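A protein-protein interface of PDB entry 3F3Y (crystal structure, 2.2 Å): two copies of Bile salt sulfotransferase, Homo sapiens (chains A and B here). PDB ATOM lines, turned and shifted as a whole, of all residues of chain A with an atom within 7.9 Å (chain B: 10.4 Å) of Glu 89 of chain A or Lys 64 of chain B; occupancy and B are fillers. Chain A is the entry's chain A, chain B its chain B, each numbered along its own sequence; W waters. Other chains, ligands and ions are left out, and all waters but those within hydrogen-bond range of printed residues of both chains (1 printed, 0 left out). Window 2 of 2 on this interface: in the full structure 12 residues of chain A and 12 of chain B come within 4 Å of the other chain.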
ATOM      1  N   PHE A  30      -3.795   7.344 -28.316  1.00  0.00           N
ATOM      2  CA  PHE A  30      -2.617   7.085 -27.476  1.00  0.00           C
ATOM      3  C   PHE A  30      -2.994   6.167 -26.300  1.00  0.00           C
ATOM      4  O   PHE A  30      -4.077   6.306 -25.665  1.00  0.00           O
ATOM      5  CB  PHE A  30      -1.955   8.395 -27.034  1.00  0.00           C
ATOM      6  CG  PHE A  30      -0.786   8.214 -26.071  1.00  0.00           C
ATOM      7  CD1 PHE A  30       0.508   8.186 -26.536  1.00  0.00           C
ATOM      8  CD2 PHE A  30      -1.002   8.094 -24.694  1.00  0.00           C
ATOM      9  CE1 PHE A  30       1.578   8.025 -25.651  1.00  0.00           C
ATOM     10  CE2 PHE A  30       0.080   7.942 -23.800  1.00  0.00           C
ATOM     11  CZ  PHE A  30       1.361   7.923 -24.296  1.00  0.00           C
ATOM     12  N   ARG A  33      -0.913   3.137 -20.052  1.00  0.00           N
ATOM     13  CA  ARG A  33      -0.698   1.885 -19.364  1.00  0.00           C
ATOM     14  C   ARG A  33      -1.023   2.134 -17.915  1.00  0.00           C
ATOM     15  O   ARG A  33      -0.929   3.253 -17.461  1.00  0.00           O
ATOM     16  CB  ARG A  33       0.746   1.399 -19.538  1.00  0.00           C
ATOM     17  CG  ARG A  33       1.255   1.447 -21.015  1.00  0.00           C
ATOM     18  CD  ARG A  33       2.727   1.059 -21.103  1.00  0.00           C
ATOM     19  NE  ARG A  33       3.298   1.305 -22.456  1.00  0.00           N
ATOM     20  CZ  ARG A  33       4.582   1.429 -22.713  1.00  0.00           C
ATOM     21  NH1 ARG A  33       5.465   1.341 -21.727  1.00  0.00           N
ATOM     22  NH2 ARG A  33       5.000   1.681 -23.958  1.00  0.00           N
ATOM     23  N   GLY A  83       7.450  13.718 -27.942  1.00  0.00           N
ATOM     24  CA  GLY A  83       7.007  12.983 -26.773  1.00  0.00           C
ATOM     25  C   GLY A  83       5.987  11.918 -27.102  1.00  0.00           C
ATOM     26  O   GLY A  83       6.046  10.832 -26.555  1.00  0.00           O
ATOM     27  N   TYR A  84       5.051  12.228 -27.999  1.00  0.00           N
ATOM     28  CA  TYR A  84       4.061  11.247 -28.456  1.00  0.00           C
ATOM     29  C   TYR A  84       4.799  10.056 -29.013  1.00  0.00           C
ATOM     30  O   TYR A  84       4.429   8.915 -28.787  1.00  0.00           O
ATOM     31  CB  TYR A  84       3.172  11.854 -29.565  1.00  0.00           C
ATOM     32  CG  TYR A  84       2.220  10.876 -30.224  1.00  0.00           C
ATOM     33  CD1 TYR A  84       1.066  10.477 -29.572  1.00  0.00           C
ATOM     34  CD2 TYR A  84       2.460  10.382 -31.526  1.00  0.00           C
ATOM     35  CE1 TYR A  84       0.180   9.587 -30.147  1.00  0.00           C
ATOM     36  CE2 TYR A  84       1.561   9.483 -32.143  1.00  0.00           C
ATOM     37  CZ  TYR A  84       0.418   9.082 -31.422  1.00  0.00           C
ATOM     38  OH  TYR A  84      -0.513   8.192 -31.960  1.00  0.00           O
ATOM     39  N   THR A  85       5.862  10.336 -29.745  1.00  0.00           N
ATOM     40  CA  THR A  85       6.547   9.324 -30.495  1.00  0.00           C
ATOM     41  C   THR A  85       7.460   8.516 -29.586  1.00  0.00           C
ATOM     42  O   THR A  85       7.554   7.302 -29.729  1.00  0.00           O
ATOM     43  CB  THR A  85       7.342   9.964 -31.624  1.00  0.00           C
ATOM     44  OG1 THR A  85       6.432  10.534 -32.572  1.00  0.00           O
ATOM     45  CG2 THR A  85       8.256   8.921 -32.345  1.00  0.00           C
ATOM     46  N   ALA A  86       8.138   9.192 -28.654  1.00  0.00           N
ATOM     47  CA  ALA A  86       9.060   8.526 -27.755  1.00  0.00           C
ATOM     48  C   ALA A  86       8.335   7.612 -26.768  1.00  0.00           C
ATOM     49  O   ALA A  86       8.804   6.524 -26.477  1.00  0.00           O
ATOM     50  CB  ALA A  86       9.890   9.525 -27.030  1.00  0.00           C
ATOM     51  N   LEU A  87       7.173   8.034 -26.291  1.00  0.00           N
ATOM     52  CA  LEU A  87       6.502   7.313 -25.229  1.00  0.00           C
ATOM     53  C   LEU A  87       6.019   5.916 -25.615  1.00  0.00           C
ATOM     54  O   LEU A  87       6.210   4.976 -24.872  1.00  0.00           O
ATOM     55  CB  LEU A  87       5.373   8.136 -24.630  1.00  0.00           C
ATOM     56  CG  LEU A  87       5.858   9.230 -23.666  1.00  0.00           C
ATOM     57  CD1 LEU A  87       4.726  10.240 -23.406  1.00  0.00           C
ATOM     58  CD2 LEU A  87       6.429   8.653 -22.350  1.00  0.00           C
ATOM     59  N   SER A  88       5.417   5.779 -26.785  1.00  0.00           N
ATOM     60  CA  SER A  88       5.000   4.461 -27.269  1.00  0.00           C
ATOM     61  C   SER A  88       6.170   3.469 -27.464  1.00  0.00           C
ATOM     62  O   SER A  88       5.942   2.266 -27.435  1.00  0.00           O
ATOM     63  CB  SER A  88       4.168   4.594 -28.537  1.00  0.00           C
ATOM     64  OG  SER A  88       4.991   4.972 -29.638  1.00  0.00           O
ATOM     65  N   GLU A  89       7.413   3.981 -27.625  1.00  0.00           N
ATOM     66  CA  GLU A  89       8.629   3.139 -27.678  1.00  0.00           C
ATOM     67  C   GLU A  89       9.320   2.911 -26.314  1.00  0.00           C
ATOM     68  O   GLU A  89      10.351   2.291 -26.246  1.00  0.00           O
ATOM     69  CB  GLU A  89       9.673   3.736 -28.661  1.00  0.00           C
ATOM     70  CG  GLU A  89       9.117   4.165 -30.014  1.00  0.00           C
ATOM     71  CD  GLU A  89       8.476   3.004 -30.801  1.00  0.00           C
ATOM     72  OE1 GLU A  89       8.951   1.841 -30.676  1.00  0.00           O
ATOM     73  OE2 GLU A  89       7.493   3.255 -31.544  1.00  0.00           O
ATOM     74  N   THR A  90       8.747   3.447 -25.254  1.00  0.00           N
ATOM     75  CA  THR A  90       9.359   3.448 -23.942  1.00  0.00           C
ATOM     76  C   THR A  90       8.734   2.344 -23.092  1.00  0.00           C
ATOM     77  O   THR A  90       7.485   2.171 -23.049  1.00  0.00           O
ATOM     78  CB  THR A  90       9.239   4.895 -23.249  1.00  0.00           C
ATOM     79  OG1 THR A  90       9.875   5.871 -24.084  1.00  0.00           O
ATOM     80  CG2 THR A  90       9.930   4.943 -21.902  1.00  0.00           C
ATOM     81  N   GLU A  91       9.606   1.583 -22.428  1.00  0.00           N
ATOM     82  CA  GLU A  91       9.187   0.534 -21.525  1.00  0.00           C
ATOM     83  C   GLU A  91       8.668   1.160 -20.230  1.00  0.00           C
ATOM     84  O   GLU A  91       9.077   2.247 -19.856  1.00  0.00           O
ATOM     85  CB  GLU A  91      10.372  -0.375 -21.194  1.00  0.00           C
ATOM     86  CG  GLU A  91      11.110  -0.933 -22.373  1.00  0.00           C
ATOM     87  CD  GLU A  91      12.058  -2.045 -21.966  1.00  0.00           C
ATOM     88  OE1 GLU A  91      11.666  -2.886 -21.123  1.00  0.00           O
ATOM     89  OE2 GLU A  91      13.195  -2.072 -22.477  1.00  0.00           O
ATOM     90  N   SER A  92       7.762   0.466 -19.558  1.00  0.00           N
ATOM     91  CA  SER A  92       7.295   0.878 -18.257  1.00  0.00           C
ATOM     92  C   SER A  92       8.388   0.751 -17.193  1.00  0.00           C
ATOM     93  O   SER A  92       9.262  -0.070 -17.310  1.00  0.00           O
ATOM     94  CB  SER A  92       6.084   0.041 -17.882  1.00  0.00           C
ATOM     95  OG  SER A  92       5.017   0.252 -18.815  1.00  0.00           O
ATOM     96  N   ARG A  94       6.626   4.405 -17.188  1.00  0.00           N
ATOM     97  CA  ARG A  94       6.839   5.662 -17.851  1.00  0.00           C
ATOM     98  C   ARG A  94       6.429   6.790 -16.975  1.00  0.00           C
ATOM     99  O   ARG A  94       5.322   6.787 -16.407  1.00  0.00           O
ATOM    100  CB  ARG A  94       6.018   5.753 -19.143  1.00  0.00           C
ATOM    101  CG  ARG A  94       6.062   4.519 -19.994  1.00  0.00           C
ATOM    102  CD  ARG A  94       5.447   4.765 -21.345  1.00  0.00           C
ATOM    103  NE  ARG A  94       4.012   4.816 -21.275  1.00  0.00           N
ATOM    104  CZ  ARG A  94       3.217   4.902 -22.349  1.00  0.00           C
ATOM    105  NH1 ARG A  94       3.721   4.967 -23.591  1.00  0.00           N
ATOM    106  NH2 ARG A  94       1.934   4.972 -22.184  1.00  0.00           N
ATOM    107  N   GLU B  52      12.859 -14.362 -21.022  1.00  0.00           N
ATOM    108  CA  GLU B  52      11.943 -13.920 -22.070  1.00  0.00           C
ATOM    109  C   GLU B  52      10.533 -13.828 -21.480  1.00  0.00           C
ATOM    110  O   GLU B  52       9.753 -12.905 -21.770  1.00  0.00           O
ATOM    111  CB  GLU B  52      11.955 -14.918 -23.212  1.00  0.00           C
ATOM    112  CG  GLU B  52      11.236 -14.424 -24.424  1.00  0.00           C
ATOM    113  CD  GLU B  52      12.145 -13.666 -25.357  1.00  0.00           C
ATOM    114  OE1 GLU B  52      12.963 -12.837 -24.901  1.00  0.00           O
ATOM    115  OE2 GLU B  52      12.020 -13.888 -26.554  1.00  0.00           O
ATOM    116  N   CYS B  55      10.503 -10.507 -19.258  1.00  0.00           N
ATOM    117  CA  CYS B  55      10.364  -9.411 -20.181  1.00  0.00           C
ATOM    118  C   CYS B  55       8.945  -9.232 -20.726  1.00  0.00           C
ATOM    119  O   CYS B  55       8.453  -8.102 -20.837  1.00  0.00           O
ATOM    120  CB  CYS B  55      11.339  -9.608 -21.338  1.00  0.00           C
ATOM    121  SG  CYS B  55      13.004  -9.381 -20.807  1.00  0.00           S
ATOM    122  N   LEU B  56       8.327 -10.329 -21.130  1.00  0.00           N
ATOM    123  CA  LEU B  56       6.950 -10.326 -21.639  1.00  0.00           C
ATOM    124  C   LEU B  56       5.915 -10.032 -20.531  1.00  0.00           C
ATOM    125  O   LEU B  56       4.883  -9.426 -20.779  1.00  0.00           O
ATOM    126  CB  LEU B  56       6.638 -11.652 -22.353  1.00  0.00           C
ATOM    127  CG  LEU B  56       7.241 -11.751 -23.774  1.00  0.00           C
ATOM    128  CD1 LEU B  56       7.245 -13.185 -24.293  1.00  0.00           C
ATOM    129  CD2 LEU B  56       6.508 -10.833 -24.760  1.00  0.00           C
ATOM    130  N   MET B  57       6.185 -10.439 -19.316  1.00  0.00           N
ATOM    131  CA  MET B  57       5.244 -10.082 -18.223  1.00  0.00           C
ATOM    132  C   MET B  57       5.273  -8.556 -17.991  1.00  0.00           C
ATOM    133  O   MET B  57       4.259  -7.930 -17.668  1.00  0.00           O
ATOM    134  CB  MET B  57       5.606 -10.804 -16.938  1.00  0.00           C
ATOM    135  CG  MET B  57       5.415 -12.349 -16.966  1.00  0.00           C
ATOM    136  SD  MET B  57       5.800 -13.134 -15.338  1.00  0.00           S
ATOM    137  CE  MET B  57       5.384 -11.802 -14.211  1.00  0.00           C
ATOM    138  N   HIS B  58       6.447  -7.979 -18.228  1.00  0.00           N
ATOM    139  CA  HIS B  58       6.691  -6.601 -17.967  1.00  0.00           C
ATOM    140  C   HIS B  58       5.972  -5.738 -18.987  1.00  0.00           C
ATOM    141  O   HIS B  58       5.451  -4.690 -18.638  1.00  0.00           O
ATOM    142  CB  HIS B  58       8.188  -6.326 -18.019  1.00  0.00           C
ATOM    143  CG  HIS B  58       8.550  -4.910 -17.698  1.00  0.00           C
ATOM    144  ND1 HIS B  58       8.266  -4.329 -16.475  1.00  0.00           N
ATOM    145  CD2 HIS B  58       9.163  -3.954 -18.438  1.00  0.00           C
ATOM    146  CE1 HIS B  58       8.692  -3.082 -16.475  1.00  0.00           C
ATOM    147  NE2 HIS B  58       9.250  -2.830 -17.651  1.00  0.00           N
ATOM    148  N   SER B  59       5.975  -6.182 -20.248  1.00  0.00           N
ATOM    149  CA  SER B  59       5.302  -5.490 -21.355  1.00  0.00           C
ATOM    150  C   SER B  59       3.901  -5.978 -21.610  1.00  0.00           C
ATOM    151  O   SER B  59       3.345  -5.707 -22.655  1.00  0.00           O
ATOM    152  CB  SER B  59       6.082  -5.656 -22.636  1.00  0.00           C
ATOM    153  OG  SER B  59       6.100  -7.008 -23.064  1.00  0.00           O
ATOM    154  N   LYS B  60       3.368  -6.740 -20.681  1.00  0.00           N
ATOM    155  CA  LYS B  60       2.018  -7.311 -20.784  1.00  0.00           C
ATOM    156  C   LYS B  60       1.674  -8.092 -22.094  1.00  0.00           C
ATOM    157  O   LYS B  60       0.514  -8.116 -22.547  1.00  0.00           O
ATOM    158  CB  LYS B  60       0.980  -6.248 -20.419  1.00  0.00           C
ATOM    159  CG  LYS B  60       1.053  -5.952 -18.938  1.00  0.00           C
ATOM    160  CD  LYS B  60       0.297  -4.767 -18.544  1.00  0.00           C
ATOM    161  CE  LYS B  60       0.034  -4.810 -17.039  1.00  0.00           C
ATOM    162  NZ  LYS B  60       1.130  -5.501 -16.321  1.00  0.00           N
ATOM    163  N   GLY B  61       2.690  -8.779 -22.641  1.00  0.00           N
ATOM    164  CA  GLY B  61       2.537  -9.660 -23.784  1.00  0.00           C
ATOM    165  C   GLY B  61       3.054  -9.030 -25.048  1.00  0.00           C
ATOM    166  O   GLY B  61       3.144  -9.680 -26.078  1.00  0.00           O
ATOM    167  N   ASP B  62       3.382  -7.749 -24.966  1.00  0.00           N
ATOM    168  CA  ASP B  62       3.765  -6.979 -26.126  1.00  0.00           C
ATOM    169  C   ASP B  62       5.216  -7.278 -26.477  1.00  0.00           C
ATOM    170  O   ASP B  62       6.135  -6.983 -25.697  1.00  0.00           O
ATOM    171  CB  ASP B  62       3.543  -5.470 -25.856  1.00  0.00           C
ATOM    172  CG  ASP B  62       3.865  -4.595 -27.050  1.00  0.00           C
ATOM    173  OD1 ASP B  62       4.543  -5.059 -27.980  1.00  0.00           O
ATOM    174  OD2 ASP B  62       3.466  -3.404 -27.032  1.00  0.00           O
ATOM    175  N   ALA B  63       5.405  -7.877 -27.654  1.00  0.00           N
ATOM    176  CA  ALA B  63       6.690  -8.365 -28.092  1.00  0.00           C
ATOM    177  C   ALA B  63       7.636  -7.292 -28.642  1.00  0.00           C
ATOM    178  O   ALA B  63       8.726  -7.624 -29.089  1.00  0.00           O
ATOM    179  CB  ALA B  63       6.499  -9.462 -29.112  1.00  0.00           C
ATOM    180  N   LYS B  64       7.225  -6.012 -28.617  1.00  0.00           N
ATOM    181  CA  LYS B  64       8.034  -4.917 -29.200  1.00  0.00           C
ATOM    182  C   LYS B  64       9.486  -4.948 -28.743  1.00  0.00           C
ATOM    183  O   LYS B  64      10.423  -4.813 -29.556  1.00  0.00           O
ATOM    184  CB  LYS B  64       7.415  -3.530 -28.874  1.00  0.00           C
ATOM    185  CG  LYS B  64       8.279  -2.348 -29.289  1.00  0.00           C
ATOM    186  CD  LYS B  64       7.715  -0.922 -28.936  1.00  0.00           C
ATOM    187  CE  LYS B  64       6.400  -0.568 -29.639  1.00  0.00           C
ATOM    188  NZ  LYS B  64       5.225  -0.642 -28.663  1.00  0.00           N
ATOM    189  N   TRP B  65       9.700  -5.097 -27.440  1.00  0.00           N
ATOM    190  CA  TRP B  65      11.059  -4.930 -26.915  1.00  0.00           C
ATOM    191  C   TRP B  65      11.906  -6.160 -26.983  1.00  0.00           C
ATOM    192  O   TRP B  65      13.091  -6.045 -27.180  1.00  0.00           O
ATOM    193  CB  TRP B  65      11.076  -4.311 -25.529  1.00  0.00           C
ATOM    194  CG  TRP B  65      10.497  -2.956 -25.531  1.00  0.00           C
ATOM    195  CD1 TRP B  65      11.137  -1.800 -25.824  1.00  0.00           C
ATOM    196  CD2 TRP B  65       9.141  -2.603 -25.234  1.00  0.00           C
ATOM    197  NE1 TRP B  65      10.283  -0.751 -25.719  1.00  0.00           N
ATOM    198  CE2 TRP B  65       9.046  -1.212 -25.358  1.00  0.00           C
ATOM    199  CE3 TRP B  65       7.997  -3.334 -24.868  1.00  0.00           C
ATOM    200  CZ2 TRP B  65       7.847  -0.520 -25.140  1.00  0.00           C
ATOM    201  CZ3 TRP B  65       6.822  -2.663 -24.656  1.00  0.00           C
ATOM    202  CH2 TRP B  65       6.747  -1.262 -24.775  1.00  0.00           C
ATOM    203  N   ILE B  66      11.287  -7.340 -26.884  1.00  0.00           N
ATOM    204  CA  ILE B  66      12.018  -8.628 -27.080  1.00  0.00           C
ATOM    205  C   ILE B  66      12.460  -8.865 -28.492  1.00  0.00           C
ATOM    206  O   ILE B  66      13.368  -9.649 -28.742  1.00  0.00           O
ATOM    207  CB  ILE B  66      11.251  -9.880 -26.540  1.00  0.00           C
ATOM    208  CG1 ILE B  66      10.056 -10.267 -27.419  1.00  0.00           C
ATOM    209  CG2 ILE B  66      10.874  -9.694 -25.084  1.00  0.00           C
ATOM    210  CD1 ILE B  66       9.179 -11.380 -26.803  1.00  0.00           C
ATOM    211  N   GLN B  67      11.842  -8.174 -29.427  1.00  0.00           N
ATOM    212  CA  GLN B  67      12.200  -8.332 -30.812  1.00  0.00           C
ATOM    213  C   GLN B  67      13.142  -7.293 -31.304  1.00  0.00           C
ATOM    214  O   GLN B  67      13.636  -7.404 -32.405  1.00  0.00           O
ATOM    215  CB  GLN B  67      10.968  -8.322 -31.658  1.00  0.00           C
ATOM    216  CG  GLN B  67      10.004  -9.374 -31.257  1.00  0.00           C
ATOM    217  CD  GLN B  67       9.259  -9.883 -32.417  1.00  0.00           C
ATOM    218  OE1 GLN B  67       8.381  -9.191 -32.963  1.00  0.00           O
ATOM    219  NE2 GLN B  67       9.603 -11.098 -32.852  1.00  0.00           N
ATOM    220  N   SER B  68      13.411  -6.285 -30.470  1.00  0.00           N
ATOM    221  CA  SER B  68      14.274  -5.185 -30.831  1.00  0.00           C
ATOM    222  C   SER B  68      15.500  -5.057 -29.937  1.00  0.00           C
ATOM    223  O   SER B  68      16.466  -4.345 -30.287  1.00  0.00           O
ATOM    224  CB  SER B  68      13.488  -3.850 -30.910  1.00  0.00           C
ATOM    225  OG  SER B  68      12.788  -3.546 -29.727  1.00  0.00           O
ATOM    226  N   VAL B  69      15.486  -5.735 -28.787  1.00  0.00           N
ATOM    227  CA  VAL B  69      16.656  -5.750 -27.917  1.00  0.00           C
ATOM    228  C   VAL B  69      17.172  -7.198 -27.622  1.00  0.00           C
ATOM    229  O   VAL B  69      16.403  -8.052 -27.135  1.00  0.00           O
ATOM    230  CB  VAL B  69      16.362  -4.979 -26.596  1.00  0.00           C
ATOM    231  CG1 VAL B  69      17.569  -4.979 -25.689  1.00  0.00           C
ATOM    232  CG2 VAL B  69      15.930  -3.554 -26.886  1.00  0.00           C
ATOM    233  N   PRO B  70      18.486  -7.448 -27.861  1.00  0.00           N
ATOM    234  CA  PRO B  70      19.153  -8.707 -27.570  1.00  0.00           C
ATOM    235  C   PRO B  70      18.861  -9.166 -26.162  1.00  0.00           C
ATOM    236  O   PRO B  70      18.892  -8.376 -25.257  1.00  0.00           O
ATOM    237  CB  PRO B  70      20.629  -8.338 -27.692  1.00  0.00           C
ATOM    238  CG  PRO B  70      20.657  -7.290 -28.724  1.00  0.00           C
ATOM    239  CD  PRO B  70      19.435  -6.460 -28.416  1.00  0.00           C
ATOM    240  N   ARG B  74      18.666  -7.259 -22.247  1.00  0.00           N
ATOM    241  CA  ARG B  74      17.425  -7.153 -21.468  1.00  0.00           C
ATOM    242  C   ARG B  74      17.565  -7.808 -20.133  1.00  0.00           C
ATOM    243  O   ARG B  74      16.796  -7.535 -19.193  1.00  0.00           O
ATOM    244  CB  ARG B  74      16.282  -7.826 -22.200  1.00  0.00           C
ATOM    245  CG  ARG B  74      16.076  -7.323 -23.592  1.00  0.00           C
ATOM    246  CD  ARG B  74      14.737  -7.842 -24.182  1.00  0.00           C
ATOM    247  NE  ARG B  74      14.923  -8.856 -25.207  1.00  0.00           N
ATOM    248  CZ  ARG B  74      14.601 -10.138 -25.115  1.00  0.00           C
ATOM    249  NH1 ARG B  74      13.976 -10.655 -24.007  1.00  0.00           N
ATOM    250  NH2 ARG B  74      14.780 -10.902 -26.163  1.00  0.00           N
ATOM    251  N   LEU B 213      -0.964 -13.781 -24.510  1.00  0.00           N
ATOM    252  CA  LEU B 213       0.106 -13.227 -25.400  1.00  0.00           C
ATOM    253  C   LEU B 213       1.502 -13.562 -24.926  1.00  0.00           C
ATOM    254  O   LEU B 213       2.419 -13.657 -25.730  1.00  0.00           O
ATOM    255  CB  LEU B 213       0.008 -11.714 -25.488  1.00  0.00           C
ATOM    256  CG  LEU B 213      -0.968 -11.124 -26.463  1.00  0.00           C
ATOM    257  CD1 LEU B 213      -1.184  -9.688 -26.053  1.00  0.00           C
ATOM    258  CD2 LEU B 213      -0.440 -11.207 -27.918  1.00  0.00           C
ATOM    259  N   ASN B 217       4.006 -15.674 -27.042  1.00  0.00           N
ATOM    260  CA  ASN B 217       5.267 -15.032 -27.448  1.00  0.00           C
ATOM    261  C   ASN B 217       6.533 -15.550 -26.752  1.00  0.00           C
ATOM    262  O   ASN B 217       7.653 -15.240 -27.183  1.00  0.00           O
ATOM    263  CB  ASN B 217       5.148 -13.507 -27.315  1.00  0.00           C
ATOM    264  CG  ASN B 217       4.266 -12.893 -28.397  1.00  0.00           C
ATOM    265  OD1 ASN B 217       4.333 -13.270 -29.573  1.00  0.00           O
ATOM    266  ND2 ASN B 217       3.461 -11.939 -28.012  1.00  0.00           N
ATOM    267  N   ASN B 226      12.958 -15.600 -33.102  1.00  0.00           N
ATOM    268  CA  ASN B 226      13.351 -14.223 -32.725  1.00  0.00           C
ATOM    269  C   ASN B 226      14.880 -13.962 -32.770  1.00  0.00           C
ATOM    270  O   ASN B 226      15.629 -14.500 -31.990  1.00  0.00           O
ATOM    271  CB  ASN B 226      12.736 -13.885 -31.354  1.00  0.00           C
ATOM    272  CG  ASN B 226      13.023 -12.458 -30.897  1.00  0.00           C
ATOM    273  OD1 ASN B 226      13.712 -11.711 -31.554  1.00  0.00           O
ATOM    274  ND2 ASN B 226      12.491 -12.096 -29.770  1.00  0.00           N
ATOM    275  N   MET B 228      16.640 -11.723 -31.700  1.00  0.00           N
ATOM    276  CA  MET B 228      17.192 -11.171 -30.447  1.00  0.00           C
ATOM    277  C   MET B 228      17.417 -12.254 -29.374  1.00  0.00           C
ATOM    278  O   MET B 228      18.321 -12.136 -28.543  1.00  0.00           O
ATOM    279  CB  MET B 228      16.289 -10.045 -29.904  1.00  0.00           C
ATOM    280  CG  MET B 228      16.164  -8.820 -30.814  1.00  0.00           C
ATOM    281  SD  MET B 228      17.780  -8.071 -31.262  1.00  0.00           S
ATOM    282  CE  MET B 228      17.300  -6.950 -32.558  1.00  0.00           C
ATOM    283  N   SER B 229      16.608 -13.315 -29.430  1.00  0.00           N
ATOM    284  CA  SER B 229      16.516 -14.302 -28.349  1.00  0.00           C
ATOM    285  C   SER B 229      17.253 -15.629 -28.599  1.00  0.00           C
ATOM    286  O   SER B 229      17.424 -16.432 -27.654  1.00  0.00           O
ATOM    287  CB  SER B 229      15.061 -14.584 -28.008  1.00  0.00           C
ATOM    288  OG  SER B 229      14.463 -13.448 -27.445  1.00  0.00           O
HETATM  289  O   HOH W   1      12.009  -6.149 -21.679  1.00  0.00           O
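The backbone carbonyl oxygen (O) of Ser 88 of chain A is in hydrogen-bond range of the side-chain amino group (NZ) of Lys 64 of chain B, 3.2 Å away. A ring nitrogen (NE2) of His 58 of chain B lies within hydrogen-bond range of the backbone carbonyl oxygen (O) of Ser 92 of chain A. NE1 of Trp 65 of chain B lies within hydrogen-bond range of O of Glu 89 of chain A (3.1 Å).
The side-chain hydroxyl (OG1) of Thr 90 of chain A is in hydrogen-bond range of the backbone carbonyl oxygen (O) of Ala 86 of chain A, at 2.7 Å. The guanidinium group (NH1) of Arg 33 of chain A sits at hydrogen-bond distance from the backbone carbonyl oxygen (O) of Thr 90 of chain A (2.6 Å). The side-chain amino group of Lys 64 of chain B is in salt-bridge range of the side-chain carboxylate of Asp 62 of chain B (3.7 Å). O of Lys 64 of chain B lies within hydrogen-bond range of OG of Ser 68 of chain B (2.7 Å). The side-chain hydroxyl (OG) of Ser 92 of chain A is in hydrogen-bond range of the guanidinium group (NH1) of Arg 33 of chain A, 3.1 Å away. The side-chain hydroxyl (OG) of Ser 88 of chain A lies within hydrogen-bond range of the backbone carbonyl oxygen (O) of Thr 85 of chain A (3.5 Å).
Among the printed residues, pairs that only touch across the chains: Arg 33 of chain A with Trp 65 of chain B, Glu 89 of chain A with Lys 64 of chain B, Thr 90 of chain A with Trp 65 of chain B, Glu 91 of chain A with His 58 of chain B and Glu 91 of chain A with Trp 65 of chain B.
Glu 89 of chain A touches two residues of chain B. Lys 64 of chain B touches just these residues of chain A: Ser 88 and Glu 89. Ala 86 of chain A touches none of the printed residues of chain B. Of chain B, only Lys 64 (3.2 Å) comes within 4 Å of Ser 88 of chain A. Of chain B, only Trp 65 comes within 4 Å of Thr 90 of chain A. Printed residues of chain A within 4 Å of Trp 65 of chain B: Arg 33 (3.5 Å), Glu 89 (3.1 Å), Thr 90 (3.4 Å) and Glu 91 (3.5 Å). Of the printed residues of chain B, Arg 33 of chain A touches Trp 65. Printed residues of chain A within 4 Å of His 58 of chain B: Glu 91 and Ser 92. The nearest residue of chain A that does not touch Lys 64 of chain B is Arg 33 of chain A (5.3 Å). The nearest printed residue of chain B that does not touch Ser 92 of chain A is Trp 65 of chain B (5.6 Å).
Of the 23 printed residues of chain B, 3 touch a printed residue of chain A. Along chain B the printed residues that touch a printed residue of chain A span positions 58 to 65. Of the 13 printed residues of chain A, 6 touch a printed residue of chain B. Printed residues of chain A that touch a printed residue of chain B: Arg 33, Ser 88, Glu 89, Thr 90, Glu 91 and Ser 92. Among the printed residues, 8 pairs touch across the chains. Among the printed residues, no Asp or Glu carboxylate lies within 4 Å of a Lys or Arg side-chain nitrogen of the other chain.
No position is printed for both chains.
Water W1 bridges OE1 of Glu 91 of chain A (3.3 Å) and SG of Cys 55 of chain B (3.5 Å).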
